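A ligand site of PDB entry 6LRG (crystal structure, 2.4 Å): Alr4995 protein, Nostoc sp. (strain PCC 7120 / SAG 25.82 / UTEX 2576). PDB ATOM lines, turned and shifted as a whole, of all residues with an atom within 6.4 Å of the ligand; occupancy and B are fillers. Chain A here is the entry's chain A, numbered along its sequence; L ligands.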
ATOM      1  N   TYR A  19      29.227 -30.092  32.149  1.00  0.00           N
ATOM      2  CA  TYR A  19      30.112 -30.458  31.045  1.00  0.00           C
ATOM      3  C   TYR A  19      30.455 -29.218  30.219  1.00  0.00           C
ATOM      4  O   TYR A  19      29.940 -28.126  30.471  1.00  0.00           O
ATOM      5  CB  TYR A  19      29.479 -31.541  30.158  1.00  0.00           C
ATOM      6  CG  TYR A  19      28.015 -31.288  29.853  1.00  0.00           C
ATOM      7  CD1 TYR A  19      27.635 -30.441  28.813  1.00  0.00           C
ATOM      8  CD2 TYR A  19      27.019 -31.899  30.598  1.00  0.00           C
ATOM      9  CE1 TYR A  19      26.290 -30.195  28.535  1.00  0.00           C
ATOM     10  CE2 TYR A  19      25.678 -31.683  30.341  1.00  0.00           C
ATOM     11  CZ  TYR A  19      25.306 -30.819  29.316  1.00  0.00           C
ATOM     12  OH  TYR A  19      23.966 -30.593  29.073  1.00  0.00           O
ATOM     13  N   ILE A  21      30.469 -27.969  26.267  1.00  0.00           N
ATOM     14  CA  ILE A  21      30.197 -28.190  24.845  1.00  0.00           C
ATOM     15  C   ILE A  21      30.072 -26.886  24.066  1.00  0.00           C
ATOM     16  O   ILE A  21      29.654 -26.875  22.928  1.00  0.00           O
ATOM     17  CB  ILE A  21      28.903 -29.028  24.606  1.00  0.00           C
ATOM     18  CG1 ILE A  21      27.696 -28.348  25.248  1.00  0.00           C
ATOM     19  CG2 ILE A  21      29.061 -30.446  25.157  1.00  0.00           C
ATOM     20  CD1 ILE A  21      26.409 -29.061  24.985  1.00  0.00           C
ATOM     21  N   ASN A  22      30.418 -25.769  24.712  1.00  0.00           N
ATOM     22  CA  ASN A  22      30.526 -24.490  24.017  1.00  0.00           C
ATOM     23  C   ASN A  22      31.531 -23.698  24.828  1.00  0.00           C
ATOM     24  O   ASN A  22      31.833 -24.087  25.946  1.00  0.00           O
ATOM     25  CB  ASN A  22      29.166 -23.776  23.867  1.00  0.00           C
ATOM     26  CG  ASN A  22      28.658 -23.179  25.157  1.00  0.00           C
ATOM     27  OD1 ASN A  22      29.352 -22.421  25.820  1.00  0.00           O
ATOM     28  ND2 ASN A  22      27.403 -23.493  25.503  1.00  0.00           N
ATOM     29  N   MET A  25      30.910 -22.533  28.648  1.00  0.00           N
ATOM     30  CA  MET A  25      30.913 -23.489  29.755  1.00  0.00           C
ATOM     31  C   MET A  25      32.326 -23.776  30.252  1.00  0.00           C
ATOM     32  O   MET A  25      32.491 -24.201  31.388  1.00  0.00           O
ATOM     33  CB  MET A  25      30.246 -24.818  29.355  1.00  0.00           C
ATOM     34  CG  MET A  25      28.931 -24.699  28.668  1.00  0.00           C
ATOM     35  SD  MET A  25      28.126 -26.283  28.320  1.00  0.00           S
ATOM     36  CE  MET A  25      27.277 -26.543  29.864  1.00  0.00           C
ATOM     37  N   ASP A  65      20.588 -28.905  30.674  1.00  0.00           N
ATOM     38  CA  ASP A  65      20.323 -27.896  29.657  1.00  0.00           C
ATOM     39  C   ASP A  65      18.892 -28.007  29.100  1.00  0.00           C
ATOM     40  O   ASP A  65      18.547 -27.369  28.097  1.00  0.00           O
ATOM     41  CB  ASP A  65      21.349 -27.986  28.530  1.00  0.00           C
ATOM     42  CG  ASP A  65      22.744 -27.555  28.979  1.00  0.00           C
ATOM     43  OD1 ASP A  65      22.851 -26.544  29.717  1.00  0.00           O
ATOM     44  OD2 ASP A  65      23.735 -28.243  28.634  1.00  0.00           O
ATOM     45  N   PHE A  68      16.999 -24.808  28.477  1.00  0.00           N
ATOM     46  CA  PHE A  68      17.106 -24.014  27.266  1.00  0.00           C
ATOM     47  C   PHE A  68      16.138 -24.566  26.219  1.00  0.00           C
ATOM     48  O   PHE A  68      16.510 -25.277  25.285  1.00  0.00           O
ATOM     49  CB  PHE A  68      18.549 -23.976  26.741  1.00  0.00           C
ATOM     50  CG  PHE A  68      19.512 -23.296  27.691  1.00  0.00           C
ATOM     51  CD1 PHE A  68      19.289 -21.990  28.094  1.00  0.00           C
ATOM     52  CD2 PHE A  68      20.634 -23.966  28.175  1.00  0.00           C
ATOM     53  CE1 PHE A  68      20.167 -21.349  28.968  1.00  0.00           C
ATOM     54  CE2 PHE A  68      21.514 -23.338  29.044  1.00  0.00           C
ATOM     55  CZ  PHE A  68      21.288 -22.028  29.438  1.00  0.00           C
ATOM     56  N   ALA A  70      14.491 -23.128  23.938  1.00  0.00           N
ATOM     57  CA  ALA A  70      14.662 -22.609  22.587  1.00  0.00           C
ATOM     58  C   ALA A  70      15.175 -23.693  21.630  1.00  0.00           C
ATOM     59  O   ALA A  70      14.848 -23.683  20.440  1.00  0.00           O
ATOM     60  CB  ALA A  70      15.608 -21.450  22.595  1.00  0.00           C
ATOM     61  N   ASN A  71      15.977 -24.627  22.142  1.00  0.00           N
ATOM     62  CA  ASN A  71      16.525 -25.676  21.297  1.00  0.00           C
ATOM     63  C   ASN A  71      15.680 -26.934  21.255  1.00  0.00           C
ATOM     64  O   ASN A  71      16.083 -27.924  20.654  1.00  0.00           O
ATOM     65  CB  ASN A  71      17.933 -26.044  21.767  1.00  0.00           C
ATOM     66  CG  ASN A  71      18.828 -24.838  21.819  1.00  0.00           C
ATOM     67  OD1 ASN A  71      19.329 -24.486  22.884  1.00  0.00           O
ATOM     68  ND2 ASN A  71      19.006 -24.170  20.674  1.00  0.00           N
ATOM     69  N   PHE A  85      20.259 -32.981  18.595  1.00  0.00           N
ATOM     70  CA  PHE A  85      21.450 -32.293  19.056  1.00  0.00           C
ATOM     71  C   PHE A  85      22.764 -32.895  18.553  1.00  0.00           C
ATOM     72  O   PHE A  85      22.917 -34.103  18.428  1.00  0.00           O
ATOM     73  CB  PHE A  85      21.468 -32.270  20.587  1.00  0.00           C
ATOM     74  CG  PHE A  85      20.329 -31.474  21.204  1.00  0.00           C
ATOM     75  CD1 PHE A  85      20.456 -30.112  21.419  1.00  0.00           C
ATOM     76  CD2 PHE A  85      19.154 -32.093  21.570  1.00  0.00           C
ATOM     77  CE1 PHE A  85      19.459 -29.393  21.976  1.00  0.00           C
ATOM     78  CE2 PHE A  85      18.127 -31.376  22.125  1.00  0.00           C
ATOM     79  CZ  PHE A  85      18.275 -30.017  22.332  1.00  0.00           C
ATOM     80  N   HIS A  87      25.703 -32.769  20.305  1.00  0.00           N
ATOM     81  CA  HIS A  87      26.417 -33.400  21.428  1.00  0.00           C
ATOM     82  C   HIS A  87      25.526 -34.340  22.222  1.00  0.00           C
ATOM     83  O   HIS A  87      24.406 -33.994  22.551  1.00  0.00           O
ATOM     84  CB  HIS A  87      26.959 -32.344  22.378  1.00  0.00           C
ATOM     85  CG  HIS A  87      27.947 -31.423  21.757  1.00  0.00           C
ATOM     86  ND1 HIS A  87      29.300 -31.713  21.697  1.00  0.00           N
ATOM     87  CD2 HIS A  87      27.792 -30.207  21.178  1.00  0.00           C
ATOM     88  CE1 HIS A  87      29.931 -30.710  21.106  1.00  0.00           C
ATOM     89  NE2 HIS A  87      29.043 -29.783  20.784  1.00  0.00           N
ATOM     90  N   ARG A  90      23.252 -33.529  25.347  1.00  0.00           N
ATOM     91  CA  ARG A  90      21.936 -32.907  25.248  1.00  0.00           C
ATOM     92  C   ARG A  90      20.939 -33.817  24.526  1.00  0.00           C
ATOM     93  O   ARG A  90      19.748 -33.556  24.526  1.00  0.00           O
ATOM     94  CB  ARG A  90      22.046 -31.562  24.522  1.00  0.00           C
ATOM     95  CG  ARG A  90      22.746 -30.470  25.325  1.00  0.00           C
ATOM     96  CD  ARG A  90      22.348 -29.089  24.825  1.00  0.00           C
ATOM     97  NE  ARG A  90      20.952 -28.784  25.148  1.00  0.00           N
ATOM     98  CZ  ARG A  90      20.355 -27.641  24.857  1.00  0.00           C
ATOM     99  NH1 ARG A  90      21.032 -26.684  24.235  1.00  0.00           N
ATOM    100  NH2 ARG A  90      19.076 -27.454  25.200  1.00  0.00           N
ATOM    101  N   GLU A 118      19.180 -27.655  15.866  1.00  0.00           N
ATOM    102  CA  GLU A 118      18.925 -27.340  17.264  1.00  0.00           C
ATOM    103  C   GLU A 118      17.858 -26.260  17.463  1.00  0.00           C
ATOM    104  O   GLU A 118      17.931 -25.431  18.367  1.00  0.00           O
ATOM    105  CB  GLU A 118      20.251 -26.986  17.951  1.00  0.00           C
ATOM    106  CG  GLU A 118      21.292 -28.112  17.766  1.00  0.00           C
ATOM    107  CD  GLU A 118      22.397 -28.178  18.849  1.00  0.00           C
ATOM    108  OE1 GLU A 118      22.540 -27.212  19.636  1.00  0.00           O
ATOM    109  OE2 GLU A 118      23.121 -29.189  18.914  1.00  0.00           O
ATOM    110  N   GLY A 121      16.521 -22.035  18.615  1.00  0.00           N
ATOM    111  CA  GLY A 121      17.812 -21.506  19.021  1.00  0.00           C
ATOM    112  C   GLY A 121      18.726 -21.188  17.854  1.00  0.00           C
ATOM    113  O   GLY A 121      19.546 -20.283  17.933  1.00  0.00           O
ATOM    114  N   ARG A 139      26.365 -25.968  15.058  1.00  0.00           N
ATOM    115  CA  ARG A 139      25.450 -26.964  15.618  1.00  0.00           C
ATOM    116  C   ARG A 139      24.559 -27.529  14.510  1.00  0.00           C
ATOM    117  O   ARG A 139      24.695 -28.679  14.112  1.00  0.00           O
ATOM    118  CB  ARG A 139      24.585 -26.375  16.741  1.00  0.00           C
ATOM    119  CG  ARG A 139      25.336 -26.039  18.032  1.00  0.00           C
ATOM    120  CD  ARG A 139      25.935 -27.291  18.704  1.00  0.00           C
ATOM    121  NE  ARG A 139      26.672 -26.948  19.913  1.00  0.00           N
ATOM    122  CZ  ARG A 139      26.117 -26.759  21.106  1.00  0.00           C
ATOM    123  NH1 ARG A 139      24.798 -26.874  21.255  1.00  0.00           N
ATOM    124  NH2 ARG A 139      26.859 -26.426  22.145  1.00  0.00           N
ATOM    125  N   TYR A 167      27.518 -19.607  18.831  1.00  0.00           N
ATOM    126  CA  TYR A 167      27.436 -20.902  18.184  1.00  0.00           C
ATOM    127  C   TYR A 167      25.975 -21.217  17.829  1.00  0.00           C
ATOM    128  O   TYR A 167      25.680 -22.220  17.176  1.00  0.00           O
ATOM    129  CB  TYR A 167      28.033 -21.979  19.107  1.00  0.00           C
ATOM    130  CG  TYR A 167      27.326 -21.993  20.429  1.00  0.00           C
ATOM    131  CD1 TYR A 167      27.630 -21.073  21.416  1.00  0.00           C
ATOM    132  CD2 TYR A 167      26.292 -22.896  20.661  1.00  0.00           C
ATOM    133  CE1 TYR A 167      26.918 -21.056  22.618  1.00  0.00           C
ATOM    134  CE2 TYR A 167      25.600 -22.891  21.842  1.00  0.00           C
ATOM    135  CZ  TYR A 167      25.914 -21.966  22.816  1.00  0.00           C
ATOM    136  OH  TYR A 167      25.210 -21.977  23.995  1.00  0.00           O
ATOM    137  N   HIS A 168      25.064 -20.376  18.292  1.00  0.00           N
ATOM    138  CA  HIS A 168      23.657 -20.463  17.914  1.00  0.00           C
ATOM    139  C   HIS A 168      23.250 -19.141  17.329  1.00  0.00           C
ATOM    140  O   HIS A 168      23.718 -18.095  17.779  1.00  0.00           O
ATOM    141  CB  HIS A 168      22.752 -20.753  19.111  1.00  0.00           C
ATOM    142  CG  HIS A 168      22.614 -22.206  19.421  1.00  0.00           C
ATOM    143  ND1 HIS A 168      22.369 -22.671  20.692  1.00  0.00           N
ATOM    144  CD2 HIS A 168      22.702 -23.298  18.627  1.00  0.00           C
ATOM    145  CE1 HIS A 168      22.310 -23.994  20.669  1.00  0.00           C
ATOM    146  NE2 HIS A 168      22.509 -24.397  19.423  1.00  0.00           N
ATOM    147  N   ASP A 170      20.611 -17.502  17.720  1.00  0.00           N
ATOM    148  CA  ASP A 170      19.900 -16.587  18.612  1.00  0.00           C
ATOM    149  C   ASP A 170      20.826 -15.909  19.617  1.00  0.00           C
ATOM    150  O   ASP A 170      20.358 -15.080  20.402  1.00  0.00           O
ATOM    151  CB  ASP A 170      18.742 -17.299  19.339  1.00  0.00           C
ATOM    152  CG  ASP A 170      19.180 -18.295  20.407  1.00  0.00           C
ATOM    153  OD1 ASP A 170      20.377 -18.646  20.483  1.00  0.00           O
ATOM    154  OD2 ASP A 170      18.293 -18.764  21.168  1.00  0.00           O
ATOM    155  N   THR A 171      22.112 -16.202  19.587  1.00  0.00           N
ATOM    156  CA  THR A 171      23.050 -15.450  20.426  1.00  0.00           C
ATOM    157  C   THR A 171      23.576 -14.189  19.728  1.00  0.00           C
ATOM    158  O   THR A 171      24.209 -13.343  20.364  1.00  0.00           O
ATOM    159  CB  THR A 171      24.276 -16.267  20.826  1.00  0.00           C
ATOM    160  OG1 THR A 171      25.093 -16.460  19.672  1.00  0.00           O
ATOM    161  CG2 THR A 171      23.878 -17.612  21.399  1.00  0.00           C
ATOM    162  N   PHE A 216      25.225 -11.048  25.738  1.00  0.00           N
ATOM    163  CA  PHE A 216      24.063 -11.690  25.129  1.00  0.00           C
ATOM    164  C   PHE A 216      22.890 -10.749  24.835  1.00  0.00           C
ATOM    165  O   PHE A 216      21.731 -11.130  25.005  1.00  0.00           O
ATOM    166  CB  PHE A 216      23.589 -12.848  26.003  1.00  0.00           C
ATOM    167  CG  PHE A 216      24.244 -14.165  25.660  1.00  0.00           C
ATOM    168  CD1 PHE A 216      25.589 -14.370  25.909  1.00  0.00           C
ATOM    169  CD2 PHE A 216      23.513 -15.198  25.109  1.00  0.00           C
ATOM    170  CE1 PHE A 216      26.186 -15.593  25.585  1.00  0.00           C
ATOM    171  CE2 PHE A 216      24.100 -16.413  24.780  1.00  0.00           C
ATOM    172  CZ  PHE A 216      25.438 -16.611  25.011  1.00  0.00           C
ATOM    173  N   ASN A 219      20.346 -12.101  22.478  1.00  0.00           N
ATOM    174  CA  ASN A 219      19.540 -13.178  23.019  1.00  0.00           C
ATOM    175  C   ASN A 219      18.341 -12.578  23.752  1.00  0.00           C
ATOM    176  O   ASN A 219      18.215 -12.660  24.968  1.00  0.00           O
ATOM    177  CB  ASN A 219      20.395 -14.061  23.943  1.00  0.00           C
ATOM    178  CG  ASN A 219      19.925 -15.516  23.978  1.00  0.00           C
ATOM    179  OD1 ASN A 219      19.686 -16.078  25.047  1.00  0.00           O
ATOM    180  ND2 ASN A 219      19.791 -16.139  22.802  1.00  0.00           N
ATOM    181  N   ALA A 258      26.653 -21.034  31.175  1.00  0.00           N
ATOM    182  CA  ALA A 258      26.407 -22.207  30.346  1.00  0.00           C
ATOM    183  C   ALA A 258      26.169 -21.827  28.874  1.00  0.00           C
ATOM    184  O   ALA A 258      25.844 -22.686  28.059  1.00  0.00           O
ATOM    185  CB  ALA A 258      25.216 -23.013  30.894  1.00  0.00           C
ATOM    186  N   GLY A 259      26.277 -20.552  28.543  1.00  0.00           N
ATOM    187  CA  GLY A 259      26.117 -20.103  27.171  1.00  0.00           C
ATOM    188  C   GLY A 259      24.738 -19.737  26.636  1.00  0.00           C
ATOM    189  O   GLY A 259      24.510 -19.789  25.437  1.00  0.00           O
ATOM    190  N   GLY A 260      23.828 -19.341  27.537  1.00  0.00           N
ATOM    191  CA  GLY A 260      22.482 -18.977  27.135  1.00  0.00           C
ATOM    192  C   GLY A 260      21.954 -17.830  27.986  1.00  0.00           C
ATOM    193  O   GLY A 260      22.509 -17.545  29.044  1.00  0.00           O
ATOM    194  N   ALA A 261      20.912 -17.159  27.499  1.00  0.00           N
ATOM    195  CA  ALA A 261      20.296 -16.072  28.246  1.00  0.00           C
ATOM    196  C   ALA A 261      18.789 -16.055  27.969  1.00  0.00           C
ATOM    197  O   ALA A 261      18.205 -17.107  27.798  1.00  0.00           O
ATOM    198  CB  ALA A 261      20.926 -14.739  27.884  1.00  0.00           C
ATOM    199  N   CYS A 264      17.258 -17.951  24.980  1.00  0.00           N
ATOM    200  CA  CYS A 264      17.569 -19.383  25.080  1.00  0.00           C
ATOM    201  C   CYS A 264      16.651 -20.131  26.040  1.00  0.00           C
ATOM    202  O   CYS A 264      16.421 -21.336  25.924  1.00  0.00           O
ATOM    203  CB  CYS A 264      19.024 -19.582  25.518  1.00  0.00           C
ATOM    204  SG  CYS A 264      20.250 -19.166  24.277  1.00  0.00           S
HETATM  205  N1  LIG L   1      24.261 -25.005  26.872  1.00  0.00           N
HETATM  206  C1  LIG L   1      23.503 -25.003  25.670  1.00  0.00           C
HETATM  207  C2  LIG L   1      23.060 -23.575  25.389  1.00  0.00           C
HETATM  208  C3  LIG L   1      22.210 -23.394  24.136  1.00  0.00           C
HETATM  209  C4  LIG L   1      21.250 -22.262  24.386  1.00  0.00           C
HETATM  210  N2  LIG L   1      21.253 -21.290  23.316  1.00  0.00           N
HETATM  211  C5  LIG L   1      24.291 -25.662  24.569  1.00  0.00           C
HETATM  212  O1  LIG L   1      25.556 -25.744  24.621  1.00  0.00           O
HETATM  213  O2  LIG L   1      23.658 -26.165  23.602  1.00  0.00           O
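SG of Cys 264 is in hydrogen-bond range of N2 of the ligand, at 2.5 Å. The guanidinium group of Arg 139 is in salt-bridge range of an oxygen (O2) of the ligand, 2.7 Å away. The guanidinium group (NH1) of Arg 90 is in salt-bridge range of an oxygen (O2) of the ligand, at 2.8 Å. ND2 of Asn 22 is in hydrogen-bond range of O1 of the ligand. The backbone carbonyl oxygen of Ala 258 is in hydrogen-bond range of a nitrogen (N1) of the ligand, at 3.0 Å. A nitrogen (N2) of the ligand lies within hydrogen-bond range of a ring nitrogen (ND1) of His 168, 3.2 Å away. A nitrogen (N1) of the ligand lies within salt-bridge range of the side-chain carboxylate (OD1) of Asp 65, at 3.5 Å. N2 of the ligand is in salt-bridge range of OD1 of Asp 170, at 3.97 Å.
SG of Cys 264 sits at hydrogen-bond distance from OD2 of Asp 170, at 3.7 Å. The side-chain hydroxyl (OH) of Tyr 167 lies within hydrogen-bond range of the side-chain amide nitrogen (ND2) of Asn 22 (3.1 Å). O of Gly 259 is in hydrogen-bond range of OH of Tyr 167 (2.7 Å). The side-chain amide oxygen (OD1) of Asn 22 sits at hydrogen-bond distance from the backbone NH (N) of Met 25 (3.2 Å). The side-chain amide nitrogen (ND2) of Asn 71 sits at hydrogen-bond distance from the backbone carbonyl oxygen (O) of Glu 118 (2.8 Å). The backbone NH of Ile 21 is in hydrogen-bond range of the side-chain sulfur of Met 25. ND2 of Asn 219 lies within hydrogen-bond range of O of Asp 170. N of Asp 170 is in hydrogen-bond range of O of Gly 121 (3.0 Å).
CG1 of Ile 21 touches O1 of the ligand (3.4 Å). Phe 68 touches the ligand. OD1 of Asn 71 touches C4 of the ligand (3.3 Å). Tyr 167 touches the ligand. Hydrophobic or aromatic side chains within 4 Å of the ligand: Ile 21, Phe 68, Tyr 167 and His 168. 12 residues have an atom within 4 Å of the ligand: Ile 21, Asn 22, Asp 65, Phe 68, Asn 71, Arg 90, Arg 139, Tyr 167, His 168, Asp 170, Ala 258 and Cys 264.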
